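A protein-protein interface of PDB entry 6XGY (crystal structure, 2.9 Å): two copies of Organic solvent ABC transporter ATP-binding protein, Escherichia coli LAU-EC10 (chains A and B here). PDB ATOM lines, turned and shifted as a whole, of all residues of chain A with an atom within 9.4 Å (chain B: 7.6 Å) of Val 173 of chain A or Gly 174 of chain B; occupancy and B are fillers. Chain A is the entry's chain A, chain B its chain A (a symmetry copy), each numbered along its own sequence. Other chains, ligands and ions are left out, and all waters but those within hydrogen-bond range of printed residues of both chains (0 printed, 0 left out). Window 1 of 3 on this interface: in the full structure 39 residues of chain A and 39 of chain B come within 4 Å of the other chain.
Of chain B, only Val 173 (3.6 Å) and Gly 174 (3.3 Å) come within 4 Å of Val 173 of chain A. Of chain A, only Ser 43, Val 173 and His 203 come within 4 Å of Gly 174 of chain B. Of the printed residues of chain A, Gln 175 of chain B touches His 203. Printed residues of chain B within 4 Å of Gly 174 of chain A: Ser 43, Val 173 and His 203. Printed residues of chain A within 4 Å of His 203 of chain B: Gly 174 (3.9 Å), Gln 175 (3.5 Å) and Asp 176 (3.9 Å). Printed residues of chain B within 4 Å of Gln 175 of chain A: His 203. The nearest residue of chain A that does not touch Gly 174 of chain B is Glu 170 of chain A (4.7 Å).
CG2 of Val 173 of chain A touches CG2 of Val 173 of chain B, at 3.6 Å. Gly 174 of chain B touches Val 173 of chain A (N to CG2, 3.3 Å). Ser 43 of chain B touches Gly 174 of chain A. N of Gly 174 of chain A touches CG2 of Val 173 of chain B, at 3.3 Å. C of Gly 174 of chain A touches ND1 of His 203 of chain B, at 3.9 Å. O of Gln 175 of chain A touches CB of His 203 of chain B, at 3.5 Å. His 203 of chain B touches Asp 176 of chain A. C of Gly 174 of chain B touches ND1 of His 203 of chain A, 3.9 Å away. Gln 175 of chain B touches His 203 of chain A. His 203 of chain A touches Asp 176 of chain B.
Of the 13 printed residues of chain B, 6 touch a printed residue of chain A. Along chain B the printed residues that touch a printed residue of chain A span positions 43 to 203.
Ser 43 of chain A touches Gly 174 of chain B, and with the chains exchanged Gly 174 of chain A touches Ser 43 of chain B. Val 173 of chain A touches its own counterpart, Val 173 of chain B. Val 173 of chain A touches Gly 174 of chain B, and with the chains exchanged Gly 174 of chain A touches Val 173 of chain B. Gly 174 of chain A touches His 203 of chain B, and with the chains exchanged His 203 of chain A touches Gly 174 of chain B. Positions printed for both chains: 43, 151, 170, 171, 172, 173, 174, 175, 176, 179, 180, 203 and 204. Of the 11 pairs that touch across the chains among the printed residues, 11 have their exchanged pair printed and touching as well.
The backbone carbonyl oxygen of Gly 41 of chain A lies within hydrogen-bond range of a ring nitrogen (NE2) of His 203 of chain A (3.3 Å). The side-chain amino group (NZ) of Lys 47 of chain A is in hydrogen-bond range of a ring nitrogen (NE2) of His 203 of chain A, at 3.1 Å. The side-chain amide nitrogen (NE2) of Gln 175 of chain A sits close to the guanidinium group (NE) of Arg 151 of chain A. The side-chain hydroxyl (OG1) of Thr 179 of chain A lies within hydrogen-bond range of the side-chain carboxylate (OD2) of Asp 176 of chain A (2.7 Å). NE2 of Gln 175 of chain B lies close to NE of Arg 151 of chain B (2.9 Å). The side-chain hydroxyl (OG1) of Thr 179 of chain B lies within hydrogen-bond range of the side-chain carboxylate (OD2) of Asp 176 of chain B.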
ATOM      1  N   GLY A  41      17.829  15.073 -12.218  1.00  0.00           N
ATOM      2  CA  GLY A  41      18.988  14.608 -12.941  1.00  0.00           C
ATOM      3  C   GLY A  41      19.560  15.673 -13.852  1.00  0.00           C
ATOM      4  O   GLY A  41      18.919  16.692 -14.128  1.00  0.00           O
ATOM      5  N   PRO A  42      20.786  15.460 -14.335  1.00  0.00           N
ATOM      6  CA  PRO A  42      21.413  16.452 -15.213  1.00  0.00           C
ATOM      7  C   PRO A  42      20.635  16.625 -16.510  1.00  0.00           C
ATOM      8  O   PRO A  42      19.852  15.767 -16.922  1.00  0.00           O
ATOM      9  CB  PRO A  42      22.809  15.870 -15.471  1.00  0.00           C
ATOM     10  CG  PRO A  42      23.045  14.926 -14.341  1.00  0.00           C
ATOM     11  CD  PRO A  42      21.701  14.350 -14.020  1.00  0.00           C
ATOM     12  N   SER A  43      20.860  17.770 -17.151  1.00  0.00           N
ATOM     13  CA  SER A  43      20.211  18.061 -18.422  1.00  0.00           C
ATOM     14  C   SER A  43      20.659  17.069 -19.489  1.00  0.00           C
ATOM     15  O   SER A  43      21.848  16.765 -19.618  1.00  0.00           O
ATOM     16  CB  SER A  43      20.537  19.488 -18.867  1.00  0.00           C
ATOM     17  OG  SER A  43      20.031  20.442 -17.950  1.00  0.00           O
ATOM     18  N   GLY A  44      19.696  16.559 -20.252  1.00  0.00           N
ATOM     19  CA  GLY A  44      19.978  15.618 -21.317  1.00  0.00           C
ATOM     20  C   GLY A  44      19.914  14.157 -20.932  1.00  0.00           C
ATOM     21  O   GLY A  44      20.254  13.302 -21.760  1.00  0.00           O
ATOM     22  N   LYS A  47      14.707  12.944 -18.967  1.00  0.00           N
ATOM     23  CA  LYS A  47      13.554  13.191 -18.108  1.00  0.00           C
ATOM     24  C   LYS A  47      12.292  13.411 -18.937  1.00  0.00           C
ATOM     25  O   LYS A  47      11.256  12.780 -18.694  1.00  0.00           O
ATOM     26  CB  LYS A  47      13.833  14.388 -17.199  1.00  0.00           C
ATOM     27  CG  LYS A  47      14.950  14.148 -16.193  1.00  0.00           C
ATOM     28  CD  LYS A  47      15.379  15.438 -15.493  1.00  0.00           C
ATOM     29  CE  LYS A  47      16.540  16.108 -16.213  1.00  0.00           C
ATOM     30  NZ  LYS A  47      16.303  17.549 -16.480  1.00  0.00           N
ATOM     31  N   PHE A  91       1.707  22.495 -18.890  1.00  0.00           N
ATOM     32  CA  PHE A  91       2.567  23.537 -19.454  1.00  0.00           C
ATOM     33  C   PHE A  91       3.122  23.103 -20.808  1.00  0.00           C
ATOM     34  O   PHE A  91       4.256  23.417 -21.174  1.00  0.00           O
ATOM     35  CB  PHE A  91       3.671  23.935 -18.478  1.00  0.00           C
ATOM     36  CG  PHE A  91       3.145  24.369 -17.139  1.00  0.00           C
ATOM     37  CD1 PHE A  91       1.899  24.968 -17.033  1.00  0.00           C
ATOM     38  CD2 PHE A  91       3.880  24.163 -15.984  1.00  0.00           C
ATOM     39  CE1 PHE A  91       1.399  25.359 -15.811  1.00  0.00           C
ATOM     40  CE2 PHE A  91       3.383  24.558 -14.751  1.00  0.00           C
ATOM     41  CZ  PHE A  91       2.141  25.157 -14.668  1.00  0.00           C
ATOM     42  N   GLY A 147       2.835  36.246 -16.603  1.00  0.00           N
ATOM     43  CA  GLY A 147       3.579  35.018 -16.818  1.00  0.00           C
ATOM     44  C   GLY A 147       3.084  33.908 -15.915  1.00  0.00           C
ATOM     45  O   GLY A 147       2.552  32.900 -16.389  1.00  0.00           O
ATOM     46  N   GLY A 148       3.218  34.110 -14.604  1.00  0.00           N
ATOM     47  CA  GLY A 148       2.767  33.100 -13.663  1.00  0.00           C
ATOM     48  C   GLY A 148       1.258  32.936 -13.645  1.00  0.00           C
ATOM     49  O   GLY A 148       0.751  31.825 -13.468  1.00  0.00           O
ATOM     50  N   ARG A 151       0.061  30.366 -16.221  1.00  0.00           N
ATOM     51  CA  ARG A 151       0.308  28.972 -15.877  1.00  0.00           C
ATOM     52  C   ARG A 151      -0.626  28.489 -14.777  1.00  0.00           C
ATOM     53  O   ARG A 151      -0.943  27.295 -14.718  1.00  0.00           O
ATOM     54  CB  ARG A 151       1.765  28.802 -15.465  1.00  0.00           C
ATOM     55  CG  ARG A 151       2.719  29.430 -16.460  1.00  0.00           C
ATOM     56  CD  ARG A 151       4.073  29.712 -15.847  1.00  0.00           C
ATOM     57  NE  ARG A 151       4.904  28.516 -15.784  1.00  0.00           N
ATOM     58  CZ  ARG A 151       5.635  28.065 -16.799  1.00  0.00           C
ATOM     59  NH1 ARG A 151       5.628  28.708 -17.959  1.00  0.00           N
ATOM     60  NH2 ARG A 151       6.369  26.972 -16.656  1.00  0.00           N
ATOM     61  N   ASP A 169       6.800  19.273 -16.371  1.00  0.00           N
ATOM     62  CA  ASP A 169       8.129  19.190 -16.977  1.00  0.00           C
ATOM     63  C   ASP A 169       8.861  20.504 -16.712  1.00  0.00           C
ATOM     64  O   ASP A 169       8.671  21.489 -17.431  1.00  0.00           O
ATOM     65  CB  ASP A 169       8.021  18.898 -18.470  1.00  0.00           C
ATOM     66  CG  ASP A 169       9.289  18.290 -19.036  1.00  0.00           C
ATOM     67  OD1 ASP A 169      10.344  18.388 -18.375  1.00  0.00           O
ATOM     68  OD2 ASP A 169       9.229  17.711 -20.143  1.00  0.00           O
ATOM     69  N   GLU A 170       9.711  20.503 -15.688  1.00  0.00           N
ATOM     70  CA  GLU A 170      10.450  21.684 -15.254  1.00  0.00           C
ATOM     71  C   GLU A 170       9.541  22.910 -15.143  1.00  0.00           C
ATOM     72  O   GLU A 170       9.764  23.921 -15.825  1.00  0.00           O
ATOM     73  CB  GLU A 170      11.625  21.959 -16.181  1.00  0.00           C
ATOM     74  CG  GLU A 170      12.654  20.836 -16.215  1.00  0.00           C
ATOM     75  CD  GLU A 170      13.868  21.172 -17.062  1.00  0.00           C
ATOM     76  OE1 GLU A 170      14.262  22.358 -17.095  1.00  0.00           O
ATOM     77  OE2 GLU A 170      14.423  20.251 -17.698  1.00  0.00           O
ATOM     78  N   PRO A 171       8.519  22.866 -14.285  1.00  0.00           N
ATOM     79  CA  PRO A 171       7.522  23.945 -14.266  1.00  0.00           C
ATOM     80  C   PRO A 171       8.009  25.238 -13.633  1.00  0.00           C
ATOM     81  O   PRO A 171       7.329  26.262 -13.773  1.00  0.00           O
ATOM     82  CB  PRO A 171       6.376  23.338 -13.451  1.00  0.00           C
ATOM     83  CG  PRO A 171       7.064  22.411 -12.507  1.00  0.00           C
ATOM     84  CD  PRO A 171       8.230  21.834 -13.271  1.00  0.00           C
ATOM     85  N   PHE A 172       9.152  25.232 -12.949  1.00  0.00           N
ATOM     86  CA  PHE A 172       9.601  26.386 -12.182  1.00  0.00           C
ATOM     87  C   PHE A 172      10.645  27.225 -12.901  1.00  0.00           C
ATOM     88  O   PHE A 172      11.085  28.239 -12.350  1.00  0.00           O
ATOM     89  CB  PHE A 172      10.171  25.933 -10.836  1.00  0.00           C
ATOM     90  CG  PHE A 172       9.240  25.072 -10.044  1.00  0.00           C
ATOM     91  CD1 PHE A 172       7.931  25.463  -9.828  1.00  0.00           C
ATOM     92  CD2 PHE A 172       9.672  23.864  -9.524  1.00  0.00           C
ATOM     93  CE1 PHE A 172       7.070  24.671  -9.098  1.00  0.00           C
ATOM     94  CE2 PHE A 172       8.816  23.064  -8.796  1.00  0.00           C
ATOM     95  CZ  PHE A 172       7.513  23.468  -8.582  1.00  0.00           C
ATOM     96  N   VAL A 173      11.058  26.835 -14.107  1.00  0.00           N
ATOM     97  CA  VAL A 173      12.205  27.480 -14.731  1.00  0.00           C
ATOM     98  C   VAL A 173      11.854  28.911 -15.113  1.00  0.00           C
ATOM     99  O   VAL A 173      10.709  29.220 -15.472  1.00  0.00           O
ATOM    100  CB  VAL A 173      12.694  26.660 -15.938  1.00  0.00           C
ATOM    101  CG1 VAL A 173      11.894  26.981 -17.187  1.00  0.00           C
ATOM    102  CG2 VAL A 173      14.177  26.887 -16.161  1.00  0.00           C
ATOM    103  N   GLY A 174      12.839  29.799 -15.003  1.00  0.00           N
ATOM    104  CA  GLY A 174      12.642  31.200 -15.319  1.00  0.00           C
ATOM    105  C   GLY A 174      11.621  31.911 -14.461  1.00  0.00           C
ATOM    106  O   GLY A 174      10.960  32.836 -14.942  1.00  0.00           O
ATOM    107  N   GLN A 175      11.470  31.510 -13.202  1.00  0.00           N
ATOM    108  CA  GLN A 175      10.456  32.073 -12.324  1.00  0.00           C
ATOM    109  C   GLN A 175      11.096  32.680 -11.085  1.00  0.00           C
ATOM    110  O   GLN A 175      12.015  32.099 -10.496  1.00  0.00           O
ATOM    111  CB  GLN A 175       9.434  31.016 -11.914  1.00  0.00           C
ATOM    112  CG  GLN A 175       8.593  30.500 -13.060  1.00  0.00           C
ATOM    113  CD  GLN A 175       7.321  29.834 -12.581  1.00  0.00           C
ATOM    114  OE1 GLN A 175       7.185  29.505 -11.402  1.00  0.00           O
ATOM    115  NE2 GLN A 175       6.376  29.643 -13.490  1.00  0.00           N
ATOM    116  N   ASP A 176      10.594  33.847 -10.692  1.00  0.00           N
ATOM    117  CA  ASP A 176      11.021  34.481  -9.464  1.00  0.00           C
ATOM    118  C   ASP A 176      10.498  33.689  -8.266  1.00  0.00           C
ATOM    119  O   ASP A 176       9.536  32.927  -8.389  1.00  0.00           O
ATOM    120  CB  ASP A 176      10.530  35.925  -9.426  1.00  0.00           C
ATOM    121  CG  ASP A 176       9.045  36.042  -9.693  1.00  0.00           C
ATOM    122  OD1 ASP A 176       8.300  36.379  -8.752  1.00  0.00           O
ATOM    123  OD2 ASP A 176       8.623  35.777 -10.840  1.00  0.00           O
ATOM    124  N   THR A 179       6.608  33.798  -7.687  1.00  0.00           N
ATOM    125  CA  THR A 179       5.863  32.998  -8.654  1.00  0.00           C
ATOM    126  C   THR A 179       6.079  31.510  -8.414  1.00  0.00           C
ATOM    127  O   THR A 179       5.132  30.716  -8.479  1.00  0.00           O
ATOM    128  CB  THR A 179       6.283  33.370 -10.075  1.00  0.00           C
ATOM    129  OG1 THR A 179       6.217  34.792 -10.239  1.00  0.00           O
ATOM    130  CG2 THR A 179       5.374  32.701 -11.094  1.00  0.00           C
ATOM    131  N   MET A 180       7.321  31.119  -8.125  1.00  0.00           N
ATOM    132  CA  MET A 180       7.628  29.715  -7.881  1.00  0.00           C
ATOM    133  C   MET A 180       6.980  29.228  -6.594  1.00  0.00           C
ATOM    134  O   MET A 180       6.397  28.139  -6.556  1.00  0.00           O
ATOM    135  CB  MET A 180       9.143  29.518  -7.830  1.00  0.00           C
ATOM    136  CG  MET A 180       9.582  28.075  -7.663  1.00  0.00           C
ATOM    137  SD  MET A 180      11.379  27.902  -7.625  1.00  0.00           S
ATOM    138  CE  MET A 180      11.834  28.791  -9.109  1.00  0.00           C
ATOM    139  N   LEU A 183       3.350  28.334  -7.108  1.00  0.00           N
ATOM    140  CA  LEU A 183       3.093  27.102  -7.845  1.00  0.00           C
ATOM    141  C   LEU A 183       3.487  25.870  -7.039  1.00  0.00           C
ATOM    142  O   LEU A 183       2.896  24.799  -7.224  1.00  0.00           O
ATOM    143  CB  LEU A 183       3.830  27.132  -9.183  1.00  0.00           C
ATOM    144  CG  LEU A 183       3.290  26.192 -10.260  1.00  0.00           C
ATOM    145  CD1 LEU A 183       1.782  26.316 -10.352  1.00  0.00           C
ATOM    146  CD2 LEU A 183       3.931  26.494 -11.605  1.00  0.00           C
ATOM    147  N   VAL A 201       9.224  16.875 -12.689  1.00  0.00           N
ATOM    148  CA  VAL A 201      10.617  16.983 -13.103  1.00  0.00           C
ATOM    149  C   VAL A 201      11.069  18.413 -12.853  1.00  0.00           C
ATOM    150  O   VAL A 201      10.368  19.363 -13.221  1.00  0.00           O
ATOM    151  CB  VAL A 201      10.780  16.607 -14.586  1.00  0.00           C
ATOM    152  CG1 VAL A 201      12.196  16.886 -15.053  1.00  0.00           C
ATOM    153  CG2 VAL A 201      10.412  15.148 -14.815  1.00  0.00           C
ATOM    154  N   SER A 202      12.230  18.578 -12.222  1.00  0.00           N
ATOM    155  CA  SER A 202      12.702  19.916 -11.892  1.00  0.00           C
ATOM    156  C   SER A 202      14.183  19.879 -11.549  1.00  0.00           C
ATOM    157  O   SER A 202      14.729  18.838 -11.174  1.00  0.00           O
ATOM    158  CB  SER A 202      11.914  20.520 -10.726  1.00  0.00           C
ATOM    159  OG  SER A 202      12.494  21.743 -10.304  1.00  0.00           O
ATOM    160  N   HIS A 203      14.822  21.042 -11.686  1.00  0.00           N
ATOM    161  CA  HIS A 203      16.178  21.254 -11.201  1.00  0.00           C
ATOM    162  C   HIS A 203      16.221  22.013  -9.886  1.00  0.00           C
ATOM    163  O   HIS A 203      17.264  22.019  -9.224  1.00  0.00           O
ATOM    164  CB  HIS A 203      17.006  22.019 -12.240  1.00  0.00           C
ATOM    165  CG  HIS A 203      17.317  21.224 -13.466  1.00  0.00           C
ATOM    166  ND1 HIS A 203      17.223  21.749 -14.737  1.00  0.00           N
ATOM    167  CD2 HIS A 203      17.725  19.943 -13.617  1.00  0.00           C
ATOM    168  CE1 HIS A 203      17.556  20.823 -15.618  1.00  0.00           C
ATOM    169  NE2 HIS A 203      17.867  19.718 -14.964  1.00  0.00           N
ATOM    170  N   ASP A 204      15.120  22.657  -9.502  1.00  0.00           N
ATOM    171  CA  ASP A 204      15.038  23.390  -8.242  1.00  0.00           C
ATOM    172  C   ASP A 204      14.890  22.370  -7.116  1.00  0.00           C
ATOM    173  O   ASP A 204      13.794  22.056  -6.646  1.00  0.00           O
ATOM    174  CB  ASP A 204      13.889  24.386  -8.286  1.00  0.00           C
ATOM    175  CG  ASP A 204      14.095  25.457  -9.340  1.00  0.00           C
ATOM    176  OD1 ASP A 204      15.144  26.136  -9.299  1.00  0.00           O
ATOM    177  OD2 ASP A 204      13.224  25.609 -10.221  1.00  0.00           O
ATOM    178  N   GLU A 207      13.113  23.217  -3.487  1.00  0.00           N
ATOM    179  CA  GLU A 207      11.676  23.464  -3.565  1.00  0.00           C
ATOM    180  C   GLU A 207      10.898  22.179  -3.822  1.00  0.00           C
ATOM    181  O   GLU A 207       9.849  21.950  -3.208  1.00  0.00           O
ATOM    182  CB  GLU A 207      11.374  24.497  -4.651  1.00  0.00           C
ATOM    183  CG  GLU A 207      11.775  25.930  -4.309  1.00  0.00           C
ATOM    184  CD  GLU A 207      13.255  26.198  -4.505  1.00  0.00           C
ATOM    185  OE1 GLU A 207      13.783  27.128  -3.860  1.00  0.00           O
ATOM    186  OE2 GLU A 207      13.892  25.481  -5.305  1.00  0.00           O
ATOM    187  N   SER B  43       9.651  38.969 -13.187  1.00  0.00           N
ATOM    188  CA  SER B  43       9.778  38.911 -14.637  1.00  0.00           C
ATOM    189  C   SER B  43       9.002  40.049 -15.286  1.00  0.00           C
ATOM    190  O   SER B  43       7.858  40.333 -14.918  1.00  0.00           O
ATOM    191  CB  SER B  43       9.268  37.567 -15.160  1.00  0.00           C
ATOM    192  OG  SER B  43      10.044  36.491 -14.662  1.00  0.00           O
ATOM    193  N   ARG B 151      28.934  27.051 -22.033  1.00  0.00           N
ATOM    194  CA  ARG B 151      28.875  28.361 -21.398  1.00  0.00           C
ATOM    195  C   ARG B 151      30.162  28.686 -20.654  1.00  0.00           C
ATOM    196  O   ARG B 151      30.515  29.863 -20.521  1.00  0.00           O
ATOM    197  CB  ARG B 151      27.675  28.416 -20.459  1.00  0.00           C
ATOM    198  CG  ARG B 151      26.404  27.930 -21.122  1.00  0.00           C
ATOM    199  CD  ARG B 151      25.361  27.508 -20.112  1.00  0.00           C
ATOM    200  NE  ARG B 151      24.649  28.651 -19.553  1.00  0.00           N
ATOM    201  CZ  ARG B 151      23.612  29.239 -20.139  1.00  0.00           C
ATOM    202  NH1 ARG B 151      23.172  28.797 -21.310  1.00  0.00           N
ATOM    203  NH2 ARG B 151      23.016  30.271 -19.560  1.00  0.00           N
ATOM    204  N   GLU B 170      20.467  36.385 -16.386  1.00  0.00           N
ATOM    205  CA  GLU B 170      19.902  35.125 -15.911  1.00  0.00           C
ATOM    206  C   GLU B 170      20.749  33.927 -16.344  1.00  0.00           C
ATOM    207  O   GLU B 170      20.260  33.035 -17.053  1.00  0.00           O
ATOM    208  CB  GLU B 170      18.461  34.969 -16.374  1.00  0.00           C
ATOM    209  CG  GLU B 170      17.527  36.050 -15.843  1.00  0.00           C
ATOM    210  CD  GLU B 170      16.077  35.820 -16.229  1.00  0.00           C
ATOM    211  OE1 GLU B 170      15.661  34.644 -16.310  1.00  0.00           O
ATOM    212  OE2 GLU B 170      15.357  36.815 -16.456  1.00  0.00           O
ATOM    213  N   PRO B 171      22.016  33.862 -15.926  1.00  0.00           N
ATOM    214  CA  PRO B 171      22.916  32.826 -16.451  1.00  0.00           C
ATOM    215  C   PRO B 171      22.654  31.432 -15.906  1.00  0.00           C
ATOM    216  O   PRO B 171      23.203  30.467 -16.451  1.00  0.00           O
ATOM    217  CB  PRO B 171      24.299  33.327 -16.025  1.00  0.00           C
ATOM    218  CG  PRO B 171      24.035  34.064 -14.757  1.00  0.00           C
ATOM    219  CD  PRO B 171      22.689  34.722 -14.933  1.00  0.00           C
ATOM    220  N   PHE B 172      21.843  31.290 -14.859  1.00  0.00           N
ATOM    221  CA  PHE B 172      21.671  30.011 -14.182  1.00  0.00           C
ATOM    222  C   PHE B 172      20.409  29.270 -14.595  1.00  0.00           C
ATOM    223  O   PHE B 172      20.170  28.166 -14.096  1.00  0.00           O
ATOM    224  CB  PHE B 172      21.648  30.219 -12.666  1.00  0.00           C
ATOM    225  CG  PHE B 172      22.831  30.968 -12.141  1.00  0.00           C
ATOM    226  CD1 PHE B 172      24.115  30.587 -12.487  1.00  0.00           C
ATOM    227  CD2 PHE B 172      22.658  32.059 -11.307  1.00  0.00           C
ATOM    228  CE1 PHE B 172      25.208  31.275 -12.004  1.00  0.00           C
ATOM    229  CE2 PHE B 172      23.746  32.755 -10.823  1.00  0.00           C
ATOM    230  CZ  PHE B 172      25.023  32.363 -11.172  1.00  0.00           C
ATOM    231  N   VAL B 173      19.596  29.839 -15.484  1.00  0.00           N
ATOM    232  CA  VAL B 173      18.280  29.269 -15.740  1.00  0.00           C
ATOM    233  C   VAL B 173      18.421  27.933 -16.454  1.00  0.00           C
ATOM    234  O   VAL B 173      19.344  27.724 -17.253  1.00  0.00           O
ATOM    235  CB  VAL B 173      17.408  30.262 -16.531  1.00  0.00           C
ATOM    236  CG1 VAL B 173      17.684  30.175 -18.021  1.00  0.00           C
ATOM    237  CG2 VAL B 173      15.940  30.027 -16.230  1.00  0.00           C
ATOM    238  N   GLY B 174      17.518  27.008 -16.138  1.00  0.00           N
ATOM    239  CA  GLY B 174      17.540  25.685 -16.729  1.00  0.00           C
ATOM    240  C   GLY B 174      18.783  24.875 -16.436  1.00  0.00           C
ATOM    241  O   GLY B 174      19.191  24.063 -17.270  1.00  0.00           O
ATOM    242  N   GLN B 175      19.397  25.069 -15.272  1.00  0.00           N
ATOM    243  CA  GLN B 175      20.644  24.401 -14.933  1.00  0.00           C
ATOM    244  C   GLN B 175      20.485  23.579 -13.663  1.00  0.00           C
ATOM    245  O   GLN B 175      19.865  24.026 -12.691  1.00  0.00           O
ATOM    246  CB  GLN B 175      21.779  25.408 -14.758  1.00  0.00           C
ATOM    247  CG  GLN B 175      22.156  26.132 -16.031  1.00  0.00           C
ATOM    248  CD  GLN B 175      23.535  26.749 -15.950  1.00  0.00           C
ATOM    249  OE1 GLN B 175      24.104  26.885 -14.866  1.00  0.00           O
ATOM    250  NE2 GLN B 175      24.087  27.117 -17.098  1.00  0.00           N
ATOM    251  N   ASP B 176      21.059  22.379 -13.679  1.00  0.00           N
ATOM    252  CA  ASP B 176      21.092  21.539 -12.502  1.00  0.00           C
ATOM    253  C   ASP B 176      22.043  22.140 -11.466  1.00  0.00           C
ATOM    254  O   ASP B 176      22.916  22.942 -11.807  1.00  0.00           O
ATOM    255  CB  ASP B 176      21.517  20.125 -12.884  1.00  0.00           C
ATOM    256  CG  ASP B 176      22.796  20.101 -13.692  1.00  0.00           C
ATOM    257  OD1 ASP B 176      23.824  19.636 -13.159  1.00  0.00           O
ATOM    258  OD2 ASP B 176      22.776  20.564 -14.854  1.00  0.00           O
ATOM    259  N   THR B 179      25.868  22.060 -12.380  1.00  0.00           N
ATOM    260  CA  THR B 179      26.232  23.031 -13.408  1.00  0.00           C
ATOM    261  C   THR B 179      26.166  24.452 -12.865  1.00  0.00           C
ATOM    262  O   THR B 179      27.047  25.275 -13.141  1.00  0.00           O
ATOM    263  CB  THR B 179      25.308  22.884 -14.617  1.00  0.00           C
ATOM    264  OG1 THR B 179      25.265  21.512 -15.025  1.00  0.00           O
ATOM    265  CG2 THR B 179      25.801  23.740 -15.773  1.00  0.00           C
ATOM    266  N   MET B 180      25.129  24.750 -12.081  1.00  0.00           N
ATOM    267  CA  MET B 180      24.977  26.085 -11.513  1.00  0.00           C
ATOM    268  C   MET B 180      26.067  26.374 -10.492  1.00  0.00           C
ATOM    269  O   MET B 180      26.658  27.460 -10.493  1.00  0.00           O
ATOM    270  CB  MET B 180      23.594  26.223 -10.879  1.00  0.00           C
ATOM    271  CG  MET B 180      23.292  27.604 -10.328  1.00  0.00           C
ATOM    272  SD  MET B 180      21.641  27.712  -9.606  1.00  0.00           S
ATOM    273  CE  MET B 180      20.645  27.066 -10.944  1.00  0.00           C
ATOM    274  N   HIS B 203      17.166  35.035 -10.935  1.00  0.00           N
ATOM    275  CA  HIS B 203      16.076  34.703 -10.028  1.00  0.00           C
ATOM    276  C   HIS B 203      16.495  33.738  -8.933  1.00  0.00           C
ATOM    277  O   HIS B 203      15.767  33.590  -7.945  1.00  0.00           O
ATOM    278  CB  HIS B 203      14.901  34.093 -10.802  1.00  0.00           C
ATOM    279  CG  HIS B 203      14.187  35.069 -11.680  1.00  0.00           C
ATOM    280  ND1 HIS B 203      13.792  34.763 -12.964  1.00  0.00           N
ATOM    281  CD2 HIS B 203      13.793  36.344 -11.458  1.00  0.00           C
ATOM    282  CE1 HIS B 203      13.189  35.810 -13.496  1.00  0.00           C
ATOM    283  NE2 HIS B 203      13.174  36.783 -12.602  1.00  0.00           N
ATOM    284  N   ASP B 204      17.639  33.074  -9.091  1.00  0.00           N
ATOM    285  CA  ASP B 204      18.154  32.148  -8.088  1.00  0.00           C
ATOM    286  C   ASP B 204      18.736  32.973  -6.943  1.00  0.00           C
ATOM    287  O   ASP B 204      19.938  33.239  -6.864  1.00  0.00           O
ATOM    288  CB  ASP B 204      19.175  31.208  -8.713  1.00  0.00           C
ATOM    289  CG  ASP B 204      18.563  30.319  -9.778  1.00  0.00           C
ATOM    290  OD1 ASP B 204      17.582  29.611  -9.468  1.00  0.00           O
ATOM    291  OD2 ASP B 204      19.045  30.342 -10.929  1.00  0.00           O
